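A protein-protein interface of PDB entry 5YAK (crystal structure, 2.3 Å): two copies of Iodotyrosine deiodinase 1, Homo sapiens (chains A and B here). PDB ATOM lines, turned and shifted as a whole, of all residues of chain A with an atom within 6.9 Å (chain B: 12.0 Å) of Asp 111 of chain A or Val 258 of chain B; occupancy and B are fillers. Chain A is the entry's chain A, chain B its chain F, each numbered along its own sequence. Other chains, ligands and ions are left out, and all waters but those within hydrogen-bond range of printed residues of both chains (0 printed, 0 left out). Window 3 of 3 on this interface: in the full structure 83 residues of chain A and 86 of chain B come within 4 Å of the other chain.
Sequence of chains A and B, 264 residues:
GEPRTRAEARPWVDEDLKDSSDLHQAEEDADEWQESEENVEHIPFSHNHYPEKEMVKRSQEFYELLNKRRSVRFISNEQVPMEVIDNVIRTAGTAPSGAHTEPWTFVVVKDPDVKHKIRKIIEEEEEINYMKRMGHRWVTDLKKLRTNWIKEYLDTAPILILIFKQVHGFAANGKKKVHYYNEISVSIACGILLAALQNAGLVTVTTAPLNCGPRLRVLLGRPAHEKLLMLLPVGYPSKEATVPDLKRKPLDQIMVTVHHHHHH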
ATOM      1  N   VAL A 107     -12.654 -12.145 -19.425  1.00  0.00           N
ATOM      2  CA  VAL A 107     -11.978 -13.134 -20.274  1.00  0.00           C
ATOM      3  C   VAL A 107     -11.271 -12.378 -21.367  1.00  0.00           C
ATOM      4  O   VAL A 107     -11.913 -11.685 -22.140  1.00  0.00           O
ATOM      5  CB  VAL A 107     -12.948 -14.120 -20.910  1.00  0.00           C
ATOM      6  CG1 VAL A 107     -12.211 -15.006 -21.904  1.00  0.00           C
ATOM      7  CG2 VAL A 107     -13.644 -14.947 -19.838  1.00  0.00           C
ATOM      8  N   VAL A 108      -9.951 -12.494 -21.370  1.00  0.00           N
ATOM      9  CA  VAL A 108      -9.079 -11.673 -22.175  1.00  0.00           C
ATOM     10  C   VAL A 108      -8.584 -12.597 -23.271  1.00  0.00           C
ATOM     11  O   VAL A 108      -8.088 -13.694 -22.983  1.00  0.00           O
ATOM     12  CB  VAL A 108      -7.873 -11.170 -21.352  1.00  0.00           C
ATOM     13  CG1 VAL A 108      -6.736 -10.711 -22.256  1.00  0.00           C
ATOM     14  CG2 VAL A 108      -8.289 -10.049 -20.431  1.00  0.00           C
ATOM     15  N   VAL A 109      -8.790 -12.191 -24.520  1.00  0.00           N
ATOM     16  CA  VAL A 109      -8.374 -13.002 -25.660  1.00  0.00           C
ATOM     17  C   VAL A 109      -7.342 -12.208 -26.481  1.00  0.00           C
ATOM     18  O   VAL A 109      -7.648 -11.116 -26.987  1.00  0.00           O
ATOM     19  CB  VAL A 109      -9.563 -13.380 -26.561  1.00  0.00           C
ATOM     20  CG1 VAL A 109      -9.094 -14.294 -27.685  1.00  0.00           C
ATOM     21  CG2 VAL A 109     -10.667 -14.065 -25.781  1.00  0.00           C
ATOM     22  N   LYS A 110      -6.133 -12.750 -26.608  1.00  0.00           N
ATOM     23  CA  LYS A 110      -5.105 -12.166 -27.509  1.00  0.00           C
ATOM     24  C   LYS A 110      -4.907 -13.026 -28.762  1.00  0.00           C
ATOM     25  O   LYS A 110      -4.442 -12.530 -29.773  1.00  0.00           O
ATOM     26  CB  LYS A 110      -3.715 -12.015 -26.844  1.00  0.00           C
ATOM     27  CG  LYS A 110      -3.644 -12.108 -25.328  1.00  0.00           C
ATOM     28  CD  LYS A 110      -2.206 -12.278 -24.842  1.00  0.00           C
ATOM     29  CE  LYS A 110      -1.740 -13.722 -24.951  1.00  0.00           C
ATOM     30  NZ  LYS A 110      -0.442 -13.913 -24.256  1.00  0.00           N
ATOM     31  N   ASP A 111      -5.216 -14.317 -28.675  1.00  0.00           N
ATOM     32  CA  ASP A 111      -4.884 -15.256 -29.747  1.00  0.00           C
ATOM     33  C   ASP A 111      -5.700 -15.052 -31.037  1.00  0.00           C
ATOM     34  O   ASP A 111      -6.933 -15.220 -31.027  1.00  0.00           O
ATOM     35  CB  ASP A 111      -5.083 -16.698 -29.288  1.00  0.00           C
ATOM     36  CG  ASP A 111      -4.783 -17.694 -30.395  1.00  0.00           C
ATOM     37  OD1 ASP A 111      -3.572 -17.925 -30.629  1.00  0.00           O
ATOM     38  OD2 ASP A 111      -5.740 -18.177 -31.063  1.00  0.00           O
ATOM     39  N   PRO A 112      -4.998 -14.791 -32.170  1.00  0.00           N
ATOM     40  CA  PRO A 112      -5.588 -14.540 -33.487  1.00  0.00           C
ATOM     41  C   PRO A 112      -6.691 -15.498 -33.901  1.00  0.00           C
ATOM     42  O   PRO A 112      -7.703 -15.054 -34.444  1.00  0.00           O
ATOM     43  CB  PRO A 112      -4.396 -14.671 -34.424  1.00  0.00           C
ATOM     44  CG  PRO A 112      -3.262 -14.146 -33.616  1.00  0.00           C
ATOM     45  CD  PRO A 112      -3.527 -14.645 -32.216  1.00  0.00           C
ATOM     46  N   ASP A 113      -6.519 -16.791 -33.633  1.00  0.00           N
ATOM     47  CA  ASP A 113      -7.444 -17.784 -34.169  1.00  0.00           C
ATOM     48  C   ASP A 113      -8.748 -17.786 -33.419  1.00  0.00           C
ATOM     49  O   ASP A 113      -9.821 -17.927 -34.017  1.00  0.00           O
ATOM     50  CB  ASP A 113      -6.801 -19.180 -34.189  1.00  0.00           C
ATOM     51  CG  ASP A 113      -5.769 -19.326 -35.320  1.00  0.00           C
ATOM     52  OD1 ASP A 113      -6.177 -19.205 -36.502  1.00  0.00           O
ATOM     53  OD2 ASP A 113      -4.563 -19.519 -35.030  1.00  0.00           O
ATOM     54  N   VAL A 114      -8.669 -17.609 -32.108  1.00  0.00           N
ATOM     55  CA  VAL A 114      -9.876 -17.603 -31.314  1.00  0.00           C
ATOM     56  C   VAL A 114     -10.626 -16.340 -31.638  1.00  0.00           C
ATOM     57  O   VAL A 114     -11.814 -16.328 -31.803  1.00  0.00           O
ATOM     58  CB  VAL A 114      -9.545 -17.606 -29.830  1.00  0.00           C
ATOM     59  CG1 VAL A 114     -10.842 -17.575 -29.015  1.00  0.00           C
ATOM     60  CG2 VAL A 114      -8.687 -18.828 -29.487  1.00  0.00           C
ATOM     61  N   LYS A 115      -9.885 -15.265 -31.757  1.00  0.00           N
ATOM     62  CA  LYS A 115     -10.439 -13.981 -32.132  1.00  0.00           C
ATOM     63  C   LYS A 115     -11.175 -14.005 -33.461  1.00  0.00           C
ATOM     64  O   LYS A 115     -12.232 -13.376 -33.610  1.00  0.00           O
ATOM     65  CB  LYS A 115      -9.331 -12.928 -32.196  1.00  0.00           C
ATOM     66  CG  LYS A 115      -8.721 -12.572 -30.849  1.00  0.00           C
ATOM     67  CD  LYS A 115      -8.298 -11.108 -30.717  1.00  0.00           C
ATOM     68  CE  LYS A 115      -7.001 -10.798 -31.437  1.00  0.00           C
ATOM     69  NZ  LYS A 115      -7.205  -9.922 -32.629  1.00  0.00           N
ATOM     70  N   HIS A 116     -10.618 -14.708 -34.438  1.00  0.00           N
ATOM     71  CA  HIS A 116     -11.277 -14.836 -35.734  1.00  0.00           C
ATOM     72  C   HIS A 116     -12.549 -15.684 -35.591  1.00  0.00           C
ATOM     73  O   HIS A 116     -13.587 -15.373 -36.223  1.00  0.00           O
ATOM     74  CB  HIS A 116     -10.308 -15.367 -36.829  1.00  0.00           C
ATOM     75  CG  HIS A 116     -10.865 -15.289 -38.228  1.00  0.00           C
ATOM     76  ND1 HIS A 116     -11.382 -14.125 -38.767  1.00  0.00           N
ATOM     77  CD2 HIS A 116     -10.996 -16.236 -39.192  1.00  0.00           C
ATOM     78  CE1 HIS A 116     -11.829 -14.365 -39.986  1.00  0.00           C
ATOM     79  NE2 HIS A 116     -11.610 -15.639 -40.266  1.00  0.00           N
ATOM     80  N   LYS A 117     -12.514 -16.690 -34.710  1.00  0.00           N
ATOM     81  CA  LYS A 117     -13.746 -17.426 -34.384  1.00  0.00           C
ATOM     82  C   LYS A 117     -14.815 -16.569 -33.669  1.00  0.00           C
ATOM     83  O   LYS A 117     -16.010 -16.686 -33.933  1.00  0.00           O
ATOM     84  CB  LYS A 117     -13.443 -18.680 -33.570  1.00  0.00           C
ATOM     85  CG  LYS A 117     -12.691 -19.775 -34.321  1.00  0.00           C
ATOM     86  CD  LYS A 117     -13.257 -21.162 -33.985  1.00  0.00           C
ATOM     87  CE  LYS A 117     -12.711 -22.257 -34.898  1.00  0.00           C
ATOM     88  NZ  LYS A 117     -11.233 -22.400 -34.785  1.00  0.00           N
ATOM     89  N   ILE A 118     -14.390 -15.678 -32.781  1.00  0.00           N
ATOM     90  CA  ILE A 118     -15.341 -14.765 -32.138  1.00  0.00           C
ATOM     91  C   ILE A 118     -16.004 -13.880 -33.196  1.00  0.00           C
ATOM     92  O   ILE A 118     -17.241 -13.717 -33.212  1.00  0.00           O
ATOM     93  CB  ILE A 118     -14.635 -13.940 -31.045  1.00  0.00           C
ATOM     94  CG1 ILE A 118     -14.294 -14.876 -29.871  1.00  0.00           C
ATOM     95  CG2 ILE A 118     -15.498 -12.758 -30.614  1.00  0.00           C
ATOM     96  CD1 ILE A 118     -13.282 -14.325 -28.908  1.00  0.00           C
ATOM     97  N   PRO A 158      -5.640  -5.925 -30.711  1.00  0.00           N
ATOM     98  CA  PRO A 158      -4.754  -6.921 -30.090  1.00  0.00           C
ATOM     99  C   PRO A 158      -5.399  -7.709 -28.926  1.00  0.00           C
ATOM    100  O   PRO A 158      -5.040  -8.865 -28.679  1.00  0.00           O
ATOM    101  CB  PRO A 158      -3.592  -6.062 -29.579  1.00  0.00           C
ATOM    102  CG  PRO A 158      -4.205  -4.716 -29.331  1.00  0.00           C
ATOM    103  CD  PRO A 158      -5.171  -4.555 -30.468  1.00  0.00           C
ATOM    104  N   LEU A 220     -15.417 -20.577 -25.433  1.00  0.00           N
ATOM    105  CA  LEU A 220     -14.303 -20.096 -24.625  1.00  0.00           C
ATOM    106  C   LEU A 220     -14.099 -20.914 -23.356  1.00  0.00           C
ATOM    107  O   LEU A 220     -13.209 -20.602 -22.572  1.00  0.00           O
ATOM    108  CB  LEU A 220     -14.493 -18.609 -24.288  1.00  0.00           C
ATOM    109  CG  LEU A 220     -14.251 -17.630 -25.433  1.00  0.00           C
ATOM    110  CD1 LEU A 220     -14.880 -16.280 -25.146  1.00  0.00           C
ATOM    111  CD2 LEU A 220     -12.762 -17.465 -25.684  1.00  0.00           C
ATOM    112  N   LEU B 251      -6.101 -11.513  -8.820  1.00  0.00           N
ATOM    113  CA  LEU B 251      -6.311 -11.343 -10.248  1.00  0.00           C
ATOM    114  C   LEU B 251      -6.600 -12.648 -11.023  1.00  0.00           C
ATOM    115  O   LEU B 251      -7.381 -12.637 -11.969  1.00  0.00           O
ATOM    116  CB  LEU B 251      -5.113 -10.608 -10.848  1.00  0.00           C
ATOM    117  CG  LEU B 251      -5.209 -10.320 -12.338  1.00  0.00           C
ATOM    118  CD1 LEU B 251      -6.463  -9.516 -12.646  1.00  0.00           C
ATOM    119  CD2 LEU B 251      -3.963  -9.585 -12.789  1.00  0.00           C
ATOM    120  N   ASP B 252      -6.004 -13.761 -10.618  1.00  0.00           N
ATOM    121  CA  ASP B 252      -6.175 -15.005 -11.350  1.00  0.00           C
ATOM    122  C   ASP B 252      -7.483 -15.696 -11.016  1.00  0.00           C
ATOM    123  O   ASP B 252      -7.777 -16.765 -11.577  1.00  0.00           O
ATOM    124  CB  ASP B 252      -4.965 -15.957 -11.177  1.00  0.00           C
ATOM    125  CG  ASP B 252      -4.775 -16.489  -9.728  1.00  0.00           C
ATOM    126  OD1 ASP B 252      -5.501 -16.114  -8.785  1.00  0.00           O
ATOM    127  OD2 ASP B 252      -3.859 -17.315  -9.533  1.00  0.00           O
ATOM    128  N   ILE B 254     -10.274 -13.621 -11.186  1.00  0.00           N
ATOM    129  CA  ILE B 254     -11.215 -12.771 -11.915  1.00  0.00           C
ATOM    130  C   ILE B 254     -10.878 -12.623 -13.387  1.00  0.00           C
ATOM    131  O   ILE B 254     -11.703 -12.126 -14.150  1.00  0.00           O
ATOM    132  CB  ILE B 254     -11.369 -11.353 -11.298  1.00  0.00           C
ATOM    133  CG1 ILE B 254     -10.146 -10.502 -11.552  1.00  0.00           C
ATOM    134  CG2 ILE B 254     -11.682 -11.431  -9.819  1.00  0.00           C
ATOM    135  CD1 ILE B 254     -10.341  -9.018 -11.250  1.00  0.00           C
ATOM    136  N   MET B 255      -9.661 -13.024 -13.770  1.00  0.00           N
ATOM    137  CA  MET B 255      -9.135 -12.811 -15.123  1.00  0.00           C
ATOM    138  C   MET B 255      -8.737 -14.158 -15.702  1.00  0.00           C
ATOM    139  O   MET B 255      -8.048 -14.920 -15.066  1.00  0.00           O
ATOM    140  CB  MET B 255      -7.920 -11.878 -15.107  1.00  0.00           C
ATOM    141  CG  MET B 255      -7.356 -11.519 -16.485  1.00  0.00           C
ATOM    142  SD  MET B 255      -5.974 -10.354 -16.390  1.00  0.00           S
ATOM    143  CE  MET B 255      -5.368 -10.342 -18.076  1.00  0.00           C
ATOM    144  N   VAL B 256      -9.193 -14.429 -16.911  1.00  0.00           N
ATOM    145  CA  VAL B 256      -8.859 -15.644 -17.647  1.00  0.00           C
ATOM    146  C   VAL B 256      -8.279 -15.193 -18.987  1.00  0.00           C
ATOM    147  O   VAL B 256      -8.897 -14.391 -19.697  1.00  0.00           O
ATOM    148  CB  VAL B 256     -10.127 -16.495 -17.858  1.00  0.00           C
ATOM    149  CG1 VAL B 256      -9.864 -17.647 -18.825  1.00  0.00           C
ATOM    150  CG2 VAL B 256     -10.606 -17.042 -16.524  1.00  0.00           C
ATOM    151  N   THR B 257      -7.070 -15.642 -19.305  1.00  0.00           N
ATOM    152  CA  THR B 257      -6.469 -15.320 -20.599  1.00  0.00           C
ATOM    153  C   THR B 257      -6.610 -16.499 -21.568  1.00  0.00           C
ATOM    154  O   THR B 257      -6.898 -17.629 -21.140  1.00  0.00           O
ATOM    155  CB  THR B 257      -5.004 -14.891 -20.448  1.00  0.00           C
ATOM    156  OG1 THR B 257      -4.922 -13.826 -19.498  1.00  0.00           O
ATOM    157  CG2 THR B 257      -4.419 -14.398 -21.771  1.00  0.00           C
ATOM    158  N   VAL B 258      -6.532 -16.203 -22.868  1.00  0.00           N
ATOM    159  CA  VAL B 258      -6.351 -17.245 -23.914  1.00  0.00           C
ATOM    160  C   VAL B 258      -5.365 -16.822 -25.027  1.00  0.00           C
ATOM    161  O   VAL B 258      -5.351 -15.667 -25.486  1.00  0.00           O
ATOM    162  CB  VAL B 258      -7.685 -17.707 -24.558  1.00  0.00           C
ATOM    163  CG1 VAL B 258      -7.454 -19.008 -25.303  1.00  0.00           C
ATOM    164  CG2 VAL B 258      -8.780 -17.903 -23.510  1.00  0.00           C
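O of Val 256 of chain B sits at hydrogen-bond distance from N of Val 108 of chain A.
O of Val 108 of chain A sits at hydrogen-bond distance from N of Val 258 of chain B (3.0 Å).
N of Lys 110 of chain A is in hydrogen-bond range of O of Val 258 of chain B (3.2 Å).
The backbone carbonyl oxygen (O) of Val 258 of chain B lies within hydrogen-bond range of the backbone NH (N) of Asp 111 of chain A (3.5 Å).
N of Asp 113 of chain A sits at hydrogen-bond distance from OD2 of Asp 111 of chain A.
N of Val 114 of chain A is in hydrogen-bond range of OD2 of Asp 111 of chain A (3.2 Å).
O of Val 256 of chain B touches CA of Val 107 of chain A, at 3.4 Å.
Met 255 of chain B touches Val 108 of chain A.
Thr 257 of chain B touches Val 108 of chain A (CA to O, 3.3 Å).
Of the printed residues of chain B, Val 107 of chain A touches Val 256 (3.4 Å).
No residue of chain B comes within 4 Å of Val 109 of chain A.
Of chain B, only Val 258 (3.2 Å) comes within 4 Å of Lys 110 of chain A.
Asp 111 of chain A touches just one residue of chain B: Val 258 (3.5 Å).
Pro 112 of chain A touches none of the printed residues of chain B.
No residue of chain B comes within 4 Å of Asp 113 of chain A.
No residue of chain B comes within 4 Å of Val 114 of chain A.
No residue of chain B comes within 4 Å of Lys 115 of chain A.
Of the printed residues of chain A, Met 255 of chain B touches Val 108 (3.8 Å).
Printed residues of chain A within 4 Å of Val 256 of chain B: Val 107 and Val 108.
Of the printed residues of chain A, Thr 257 of chain B touches Val 108.
Of chain A, only Val 108 (3.0 Å), Lys 110 (3.2 Å) and Asp 111 (3.5 Å) come within 4 Å of Val 258 of chain B.
The nearest residue of chain A that does not touch Val 258 of chain B is Val 109 of chain A (4.03 Å).
Hydrophobic or aromatic side chains of chain A that line the printed part of chain B: Val 108.
No position is printed for both chains.
Of the 7 pairs that touch across the chains among the printed residues, none has its exchanged pair printed and touching as well.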
